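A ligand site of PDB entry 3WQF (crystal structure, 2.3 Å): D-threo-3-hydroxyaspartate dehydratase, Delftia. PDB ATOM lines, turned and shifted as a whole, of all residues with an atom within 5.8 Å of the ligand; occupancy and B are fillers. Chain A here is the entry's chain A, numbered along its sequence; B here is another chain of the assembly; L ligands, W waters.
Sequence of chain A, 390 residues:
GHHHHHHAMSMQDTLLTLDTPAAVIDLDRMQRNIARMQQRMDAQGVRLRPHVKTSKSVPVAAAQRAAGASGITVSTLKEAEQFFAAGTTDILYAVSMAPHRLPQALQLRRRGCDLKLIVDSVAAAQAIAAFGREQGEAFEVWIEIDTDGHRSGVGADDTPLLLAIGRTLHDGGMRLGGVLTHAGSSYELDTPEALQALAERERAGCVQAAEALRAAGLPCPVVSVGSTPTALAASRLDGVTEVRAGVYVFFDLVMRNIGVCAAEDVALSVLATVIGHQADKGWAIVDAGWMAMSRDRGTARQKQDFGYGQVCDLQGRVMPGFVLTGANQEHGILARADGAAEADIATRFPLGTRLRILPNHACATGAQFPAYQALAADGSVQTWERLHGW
Water W1 lies within hydrogen-bond range of an oxygen (O5) of the ligand (2.7 Å), the side-chain hydroxyl of Thr 54 (2.8 Å) and the backbone NH of Val 247 (3.1 Å).
Water W2 lies within hydrogen-bond range of a ring nitrogen (NE2) of His 51 (2.8 Å), the backbone carbonyl oxygen (O) of Ala 94 (3.0 Å) and an oxygen (O1) of the ligand (3.1 Å).
NZ of Lys 53 is covalently linked to C5 of the ligand, 1.5 Å away.
N of Thr 228 sits at hydrogen-bond distance from O4 of the ligand (2.9 Å).
The side-chain hydroxyl of Thr 228 lies within hydrogen-bond range of an oxygen (O3) of the ligand, 2.6 Å away.
N of Gly 246 sits at hydrogen-bond distance from O3 of the ligand (2.6 Å).
The guanidinium group (NH2) of Arg 244 sits at hydrogen-bond distance from a nitrogen (N1) of the ligand (2.8 Å).
The side-chain hydroxyl (OH) of Tyr 187 lies within hydrogen-bond range of an oxygen (O4) of the ligand (2.9 Å).
N of Val 247 sits at hydrogen-bond distance from O3 of the ligand, at 3.1 Å.
NH2 of Arg 151 sits at hydrogen-bond distance from O1 of the ligand, 3.4 Å away.
A ring nitrogen (ND1) of His 182 is in hydrogen-bond range of a nitrogen (N1) of the ligand (3.5 Å).
OG1 of Thr 228 sits at hydrogen-bond distance from N of Tyr 248 (3.3 Å).
OG1 of Thr 54 lies close to O of Gly 246, 3.3 Å away.
The guanidinium group (NH2) of Arg 244 is in hydrogen-bond range of the backbone carbonyl oxygen (O) of Thr 181 (2.9 Å).
N of Val 247 is in hydrogen-bond range of OG1 of Thr 54 (3.1 Å).
ND1 of His 51 sits at hydrogen-bond distance from O of Thr 73, 3.4 Å away.
The guanidinium group of Arg 151 sits close to a ring nitrogen (ND1) of His 331 of chain B, 3.4 Å away.
A ring nitrogen (ND1) of His 182 sits at hydrogen-bond distance from the backbone carbonyl oxygen (O) of Gly 226, at 2.6 Å.
The side-chain hydroxyl of Ser 186 is in hydrogen-bond range of the side-chain hydroxyl of Ser 227 (3.2 Å).
His 51 touches the ligand (CD2 to C4, 3.3 Å).
CB of Ala 94 touches C2 of the ligand, 3.7 Å away.
O of Gly 226 touches C7 of the ligand, at 3.6 Å.
Ser 227 touches the ligand.
Pro 229 touches the ligand (CD to O4, 3.9 Å).
Ala 245 touches the ligand (C to O3, 3.6 Å).
Of the 24 residues printed, 14 come within 4 Å of the ligand.
The nearest printed residue that does not touch the ligand is Tyr 248 (4.7 Å).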
ATOM      1  N   HIS A  51      21.448 -20.599 -33.018  1.00  0.00           N
ATOM      2  CA  HIS A  51      21.625 -20.444 -31.590  1.00  0.00           C
ATOM      3  C   HIS A  51      22.843 -21.227 -31.123  1.00  0.00           C
ATOM      4  O   HIS A  51      22.888 -22.490 -31.166  1.00  0.00           O
ATOM      5  CB  HIS A  51      20.359 -20.870 -30.839  1.00  0.00           C
ATOM      6  CG  HIS A  51      20.169 -20.151 -29.577  1.00  0.00           C
ATOM      7  ND1 HIS A  51      21.170 -19.976 -28.702  1.00  0.00           N
ATOM      8  CD2 HIS A  51      19.102 -19.489 -29.071  1.00  0.00           C
ATOM      9  CE1 HIS A  51      20.739 -19.231 -27.686  1.00  0.00           C
ATOM     10  NE2 HIS A  51      19.468 -18.944 -27.919  1.00  0.00           N
ATOM     11  N   LYS A  53      23.837 -21.621 -28.174  1.00  0.00           N
ATOM     12  CA  LYS A  53      23.768 -22.200 -26.820  1.00  0.00           C
ATOM     13  C   LYS A  53      23.950 -23.696 -26.840  1.00  0.00           C
ATOM     14  O   LYS A  53      24.245 -24.293 -25.800  1.00  0.00           O
ATOM     15  CB  LYS A  53      22.450 -21.881 -26.095  1.00  0.00           C
ATOM     16  CG  LYS A  53      21.245 -22.680 -26.599  1.00  0.00           C
ATOM     17  CD  LYS A  53      20.038 -22.239 -25.744  1.00  0.00           C
ATOM     18  CE  LYS A  53      18.798 -23.120 -25.970  1.00  0.00           C
ATOM     19  NZ  LYS A  53      17.765 -22.343 -26.710  1.00  0.00           N
ATOM     20  N   THR A  54      23.728 -24.324 -27.999  1.00  0.00           N
ATOM     21  CA  THR A  54      23.980 -25.748 -28.089  1.00  0.00           C
ATOM     22  C   THR A  54      25.462 -26.141 -27.876  1.00  0.00           C
ATOM     23  O   THR A  54      25.718 -27.061 -27.121  1.00  0.00           O
ATOM     24  CB  THR A  54      23.514 -26.320 -29.450  1.00  0.00           C
ATOM     25  OG1 THR A  54      22.082 -26.195 -29.514  1.00  0.00           O
ATOM     26  CG2 THR A  54      23.904 -27.855 -29.497  1.00  0.00           C
ATOM     27  N   THR A  73      22.447 -16.306 -32.317  1.00  0.00           N
ATOM     28  CA  THR A  73      21.598 -15.971 -31.189  1.00  0.00           C
ATOM     29  C   THR A  73      22.346 -16.495 -29.999  1.00  0.00           C
ATOM     30  O   THR A  73      23.032 -17.541 -30.122  1.00  0.00           O
ATOM     31  CB  THR A  73      20.280 -16.754 -31.222  1.00  0.00           C
ATOM     32  OG1 THR A  73      19.650 -16.623 -32.500  1.00  0.00           O
ATOM     33  CG2 THR A  73      19.347 -16.276 -30.132  1.00  0.00           C
ATOM     34  N   ALA A  94      18.761 -13.524 -26.962  1.00  0.00           N
ATOM     35  CA  ALA A  94      17.307 -13.811 -26.985  1.00  0.00           C
ATOM     36  C   ALA A  94      16.782 -14.286 -25.630  1.00  0.00           C
ATOM     37  O   ALA A  94      16.282 -15.394 -25.518  1.00  0.00           O
ATOM     38  CB  ALA A  94      16.993 -14.824 -28.060  1.00  0.00           C
ATOM     39  N   GLU A 144       9.317  -9.850 -27.849  1.00  0.00           N
ATOM     40  CA  GLU A 144       9.070 -11.280 -27.788  1.00  0.00           C
ATOM     41  C   GLU A 144       7.580 -11.560 -27.850  1.00  0.00           C
ATOM     42  O   GLU A 144       6.766 -10.951 -27.144  1.00  0.00           O
ATOM     43  CB  GLU A 144       9.763 -11.991 -26.561  1.00  0.00           C
ATOM     44  CG  GLU A 144       9.668 -13.516 -26.589  1.00  0.00           C
ATOM     45  CD  GLU A 144      10.544 -14.293 -25.578  1.00  0.00           C
ATOM     46  OE1 GLU A 144      10.957 -15.442 -25.919  1.00  0.00           O
ATOM     47  OE2 GLU A 144      10.806 -13.814 -24.467  1.00  0.00           O
ATOM     48  N   ARG A 151       6.514 -20.026 -22.507  1.00  0.00           N
ATOM     49  CA  ARG A 151       7.563 -19.349 -21.700  1.00  0.00           C
ATOM     50  C   ARG A 151       7.240 -17.866 -21.460  1.00  0.00           C
ATOM     51  O   ARG A 151       6.304 -17.539 -20.714  1.00  0.00           O
ATOM     52  CB  ARG A 151       8.960 -19.541 -22.365  1.00  0.00           C
ATOM     53  CG  ARG A 151      10.162 -19.637 -21.423  1.00  0.00           C
ATOM     54  CD  ARG A 151      11.312 -20.418 -22.064  1.00  0.00           C
ATOM     55  NE  ARG A 151      11.935 -19.666 -23.173  1.00  0.00           N
ATOM     56  CZ  ARG A 151      12.803 -20.166 -24.072  1.00  0.00           C
ATOM     57  NH1 ARG A 151      13.171 -21.451 -24.026  1.00  0.00           N
ATOM     58  NH2 ARG A 151      13.325 -19.381 -25.019  1.00  0.00           N
ATOM     59  N   LEU A 180      10.059 -11.452 -32.381  1.00  0.00           N
ATOM     60  CA  LEU A 180      10.499 -12.823 -32.447  1.00  0.00           C
ATOM     61  C   LEU A 180       9.643 -13.712 -31.605  1.00  0.00           C
ATOM     62  O   LEU A 180       9.016 -13.248 -30.697  1.00  0.00           O
ATOM     63  CB  LEU A 180      11.951 -12.985 -32.032  1.00  0.00           C
ATOM     64  CG  LEU A 180      12.293 -13.097 -30.544  1.00  0.00           C
ATOM     65  CD1 LEU A 180      13.719 -13.646 -30.491  1.00  0.00           C
ATOM     66  CD2 LEU A 180      12.153 -11.688 -29.891  1.00  0.00           C
ATOM     67  N   THR A 181       9.667 -14.995 -31.933  1.00  0.00           N
ATOM     68  CA  THR A 181       8.969 -15.989 -31.136  1.00  0.00           C
ATOM     69  C   THR A 181       9.733 -17.262 -31.094  1.00  0.00           C
ATOM     70  O   THR A 181      10.495 -17.549 -32.025  1.00  0.00           O
ATOM     71  CB  THR A 181       7.530 -16.270 -31.653  1.00  0.00           C
ATOM     72  OG1 THR A 181       6.834 -17.068 -30.690  1.00  0.00           O
ATOM     73  CG2 THR A 181       7.538 -16.992 -32.995  1.00  0.00           C
ATOM     74  N   HIS A 182       9.534 -18.028 -30.027  1.00  0.00           N
ATOM     75  CA  HIS A 182      10.167 -19.369 -29.960  1.00  0.00           C
ATOM     76  C   HIS A 182       9.158 -20.341 -29.461  1.00  0.00           C
ATOM     77  O   HIS A 182       8.699 -20.283 -28.310  1.00  0.00           O
ATOM     78  CB  HIS A 182      11.413 -19.338 -29.089  1.00  0.00           C
ATOM     79  CG  HIS A 182      12.014 -20.694 -28.825  1.00  0.00           C
ATOM     80  ND1 HIS A 182      12.617 -21.421 -29.764  1.00  0.00           N
ATOM     81  CD2 HIS A 182      12.189 -21.396 -27.616  1.00  0.00           C
ATOM     82  CE1 HIS A 182      13.106 -22.541 -29.215  1.00  0.00           C
ATOM     83  NE2 HIS A 182      12.869 -22.509 -27.888  1.00  0.00           N
ATOM     84  N   SER A 186       7.185 -27.467 -29.284  1.00  0.00           N
ATOM     85  CA  SER A 186       7.645 -28.447 -30.335  1.00  0.00           C
ATOM     86  C   SER A 186       8.183 -29.661 -29.694  1.00  0.00           C
ATOM     87  O   SER A 186       7.974 -30.795 -30.135  1.00  0.00           O
ATOM     88  CB  SER A 186       8.759 -27.861 -31.265  1.00  0.00           C
ATOM     89  OG  SER A 186       9.816 -27.242 -30.537  1.00  0.00           O
ATOM     90  N   TYR A 187       8.890 -29.438 -28.615  1.00  0.00           N
ATOM     91  CA  TYR A 187       9.609 -30.548 -27.964  1.00  0.00           C
ATOM     92  C   TYR A 187       8.694 -31.667 -27.481  1.00  0.00           C
ATOM     93  O   TYR A 187       9.145 -32.781 -27.273  1.00  0.00           O
ATOM     94  CB  TYR A 187      10.470 -30.006 -26.824  1.00  0.00           C
ATOM     95  CG  TYR A 187      11.797 -29.405 -27.275  1.00  0.00           C
ATOM     96  CD1 TYR A 187      11.888 -28.530 -28.367  1.00  0.00           C
ATOM     97  CD2 TYR A 187      12.971 -29.724 -26.562  1.00  0.00           C
ATOM     98  CE1 TYR A 187      13.111 -27.988 -28.757  1.00  0.00           C
ATOM     99  CE2 TYR A 187      14.206 -29.193 -26.930  1.00  0.00           C
ATOM    100  CZ  TYR A 187      14.282 -28.341 -28.035  1.00  0.00           C
ATOM    101  OH  TYR A 187      15.537 -27.867 -28.390  1.00  0.00           O
ATOM    102  N   GLY A 226      11.460 -19.636 -34.546  1.00  0.00           N
ATOM    103  CA  GLY A 226      12.128 -20.928 -34.685  1.00  0.00           C
ATOM    104  C   GLY A 226      12.437 -21.733 -33.435  1.00  0.00           C
ATOM    105  O   GLY A 226      12.638 -21.186 -32.335  1.00  0.00           O
ATOM    106  N   SER A 227      12.450 -23.047 -33.648  1.00  0.00           N
ATOM    107  CA  SER A 227      13.058 -24.043 -32.803  1.00  0.00           C
ATOM    108  C   SER A 227      13.563 -24.993 -33.889  1.00  0.00           C
ATOM    109  O   SER A 227      13.197 -24.837 -35.082  1.00  0.00           O
ATOM    110  CB  SER A 227      12.029 -24.754 -31.924  1.00  0.00           C
ATOM    111  OG  SER A 227      11.029 -25.339 -32.762  1.00  0.00           O
ATOM    112  N   THR A 228      14.386 -25.959 -33.519  1.00  0.00           N
ATOM    113  CA  THR A 228      14.861 -26.906 -34.497  1.00  0.00           C
ATOM    114  C   THR A 228      13.725 -27.713 -35.185  1.00  0.00           C
ATOM    115  O   THR A 228      13.700 -27.791 -36.413  1.00  0.00           O
ATOM    116  CB  THR A 228      15.957 -27.768 -33.899  1.00  0.00           C
ATOM    117  OG1 THR A 228      17.163 -26.997 -33.962  1.00  0.00           O
ATOM    118  CG2 THR A 228      16.120 -29.131 -34.682  1.00  0.00           C
ATOM    119  N   PRO A 229      12.786 -28.264 -34.402  1.00  0.00           N
ATOM    120  CA  PRO A 229      11.664 -28.943 -35.011  1.00  0.00           C
ATOM    121  C   PRO A 229      10.756 -28.033 -35.845  1.00  0.00           C
ATOM    122  O   PRO A 229      10.309 -28.441 -36.950  1.00  0.00           O
ATOM    123  CB  PRO A 229      10.908 -29.519 -33.807  1.00  0.00           C
ATOM    124  CG  PRO A 229      11.949 -29.632 -32.724  1.00  0.00           C
ATOM    125  CD  PRO A 229      12.833 -28.441 -32.930  1.00  0.00           C
ATOM    126  N   ARG A 244      15.659 -18.972 -36.218  1.00  0.00           N
ATOM    127  CA  ARG A 244      16.691 -19.363 -35.226  1.00  0.00           C
ATOM    128  C   ARG A 244      16.555 -20.845 -34.853  1.00  0.00           C
ATOM    129  O   ARG A 244      15.451 -21.301 -34.543  1.00  0.00           O
ATOM    130  CB  ARG A 244      16.497 -18.513 -33.946  1.00  0.00           C
ATOM    131  CG  ARG A 244      16.481 -17.009 -34.243  1.00  0.00           C
ATOM    132  CD  ARG A 244      16.130 -16.191 -32.965  1.00  0.00           C
ATOM    133  NE  ARG A 244      15.276 -16.926 -31.998  1.00  0.00           N
ATOM    134  CZ  ARG A 244      13.964 -17.073 -32.130  1.00  0.00           C
ATOM    135  NH1 ARG A 244      13.308 -16.492 -33.170  1.00  0.00           N
ATOM    136  NH2 ARG A 244      13.285 -17.805 -31.239  1.00  0.00           N
ATOM    137  N   ALA A 245      17.668 -21.599 -34.891  1.00  0.00           N
ATOM    138  CA  ALA A 245      17.720 -22.999 -34.523  1.00  0.00           C
ATOM    139  C   ALA A 245      19.141 -23.230 -34.012  1.00  0.00           C
ATOM    140  O   ALA A 245      20.096 -22.626 -34.508  1.00  0.00           O
ATOM    141  CB  ALA A 245      17.434 -23.903 -35.714  1.00  0.00           C
ATOM    142  N   GLY A 246      19.257 -24.155 -33.059  1.00  0.00           N
ATOM    143  CA  GLY A 246      20.535 -24.434 -32.443  1.00  0.00           C
ATOM    144  C   GLY A 246      20.886 -25.921 -32.372  1.00  0.00           C
ATOM    145  O   GLY A 246      21.974 -26.330 -32.834  1.00  0.00           O
ATOM    146  N   VAL A 247      20.008 -26.724 -31.749  1.00  0.00           N
ATOM    147  CA  VAL A 247      20.389 -28.091 -31.381  1.00  0.00           C
ATOM    148  C   VAL A 247      20.656 -28.991 -32.657  1.00  0.00           C
ATOM    149  O   VAL A 247      21.421 -29.998 -32.623  1.00  0.00           O
ATOM    150  CB  VAL A 247      19.364 -28.705 -30.434  1.00  0.00           C
ATOM    151  CG1 VAL A 247      18.043 -29.029 -31.154  1.00  0.00           C
ATOM    152  CG2 VAL A 247      19.936 -29.979 -29.781  1.00  0.00           C
ATOM    153  N   TYR A 248      20.119 -28.558 -33.787  1.00  0.00           N
ATOM    154  CA  TYR A 248      20.187 -29.289 -35.051  1.00  0.00           C
ATOM    155  C   TYR A 248      21.607 -29.545 -35.452  1.00  0.00           C
ATOM    156  O   TYR A 248      21.868 -30.500 -36.211  1.00  0.00           O
ATOM    157  CB  TYR A 248      19.476 -28.511 -36.178  1.00  0.00           C
ATOM    158  CG  TYR A 248      20.363 -27.405 -36.707  1.00  0.00           C
ATOM    159  CD1 TYR A 248      20.417 -26.181 -36.071  1.00  0.00           C
ATOM    160  CD2 TYR A 248      21.249 -27.650 -37.781  1.00  0.00           C
ATOM    161  CE1 TYR A 248      21.263 -25.197 -36.509  1.00  0.00           C
ATOM    162  CE2 TYR A 248      22.124 -26.671 -38.211  1.00  0.00           C
ATOM    163  CZ  TYR A 248      22.082 -25.421 -37.580  1.00  0.00           C
ATOM    164  OH  TYR A 248      22.942 -24.416 -38.015  1.00  0.00           O
ATOM    165  N   MET A 255      15.369 -35.173 -30.177  1.00  0.00           N
ATOM    166  CA  MET A 255      15.063 -34.814 -31.579  1.00  0.00           C
ATOM    167  C   MET A 255      14.755 -36.040 -32.389  1.00  0.00           C
ATOM    168  O   MET A 255      13.824 -36.028 -33.167  1.00  0.00           O
ATOM    169  CB  MET A 255      16.254 -34.070 -32.217  1.00  0.00           C
ATOM    170  CG  MET A 255      16.454 -32.684 -31.592  1.00  0.00           C
ATOM    171  SD  MET A 255      15.089 -31.532 -31.951  1.00  0.00           S
ATOM    172  CE  MET A 255      14.819 -30.838 -30.348  1.00  0.00           C
ATOM    173  N   CYS A 363      22.420 -30.048 -25.822  1.00  0.00           N
ATOM    174  CA  CYS A 363      22.735 -28.805 -25.122  1.00  0.00           C
ATOM    175  C   CYS A 363      23.187 -29.131 -23.675  1.00  0.00           C
ATOM    176  O   CYS A 363      24.179 -28.567 -23.164  1.00  0.00           O
ATOM    177  CB  CYS A 363      21.549 -27.741 -25.198  1.00  0.00           C
ATOM    178  SG  CYS A 363      20.841 -27.578 -26.923  1.00  0.00           S
ATOM    179  N   HIS B 331      15.971 -20.076 -18.512  1.00  0.00           N
ATOM    180  CA  HIS B 331      14.687 -19.525 -17.948  1.00  0.00           C
ATOM    181  C   HIS B 331      14.174 -20.486 -16.913  1.00  0.00           C
ATOM    182  O   HIS B 331      13.989 -21.684 -17.215  1.00  0.00           O
ATOM    183  CB  HIS B 331      13.533 -19.475 -18.968  1.00  0.00           C
ATOM    184  CG  HIS B 331      13.738 -18.535 -20.113  1.00  0.00           C
ATOM    185  ND1 HIS B 331      14.573 -18.812 -21.141  1.00  0.00           N
ATOM    186  CD2 HIS B 331      13.132 -17.307 -20.425  1.00  0.00           C
ATOM    187  CE1 HIS B 331      14.540 -17.793 -22.035  1.00  0.00           C
ATOM    188  NE2 HIS B 331      13.647 -16.872 -21.591  1.00  0.00           N
HETATM  189  N1  LIG L   1      15.335 -19.244 -30.080  1.00  0.00           N
HETATM  190  C1  LIG L   1      15.380 -19.114 -28.764  1.00  0.00           C
HETATM  191  C2  LIG L   1      14.883 -17.862 -28.063  1.00  0.00           C
HETATM  192  C3  LIG L   1      16.014 -20.253 -28.010  1.00  0.00           C
HETATM  193  O1  LIG L   1      16.124 -20.200 -26.682  1.00  0.00           O
HETATM  194  C4  LIG L   1      16.511 -21.451 -28.735  1.00  0.00           C
HETATM  195  C5  LIG L   1      17.117 -22.590 -28.082  1.00  0.00           C
HETATM  196  C6  LIG L   1      16.355 -21.486 -30.198  1.00  0.00           C
HETATM  197  C7  LIG L   1      15.797 -20.345 -30.796  1.00  0.00           C
HETATM  198  C8  LIG L   1      16.840 -22.750 -30.925  1.00  0.00           C
HETATM  199  O2  LIG L   1      16.017 -23.836 -30.421  1.00  0.00           O
HETATM  200  P1  LIG L   1      16.410 -25.405 -30.647  1.00  0.00           P
HETATM  201  O3  LIG L   1      17.260 -25.404 -31.908  1.00  0.00           O
HETATM  202  O4  LIG L   1      15.159 -26.176 -30.755  1.00  0.00           O
HETATM  203  O5  LIG L   1      17.247 -25.567 -29.472  1.00  0.00           O
HETATM  204  O   HOH W   1      19.792 -24.613 -29.531  1.00  0.00           O
HETATM  205  O   HOH W   2      17.923 -17.850 -25.838  1.00  0.00           O
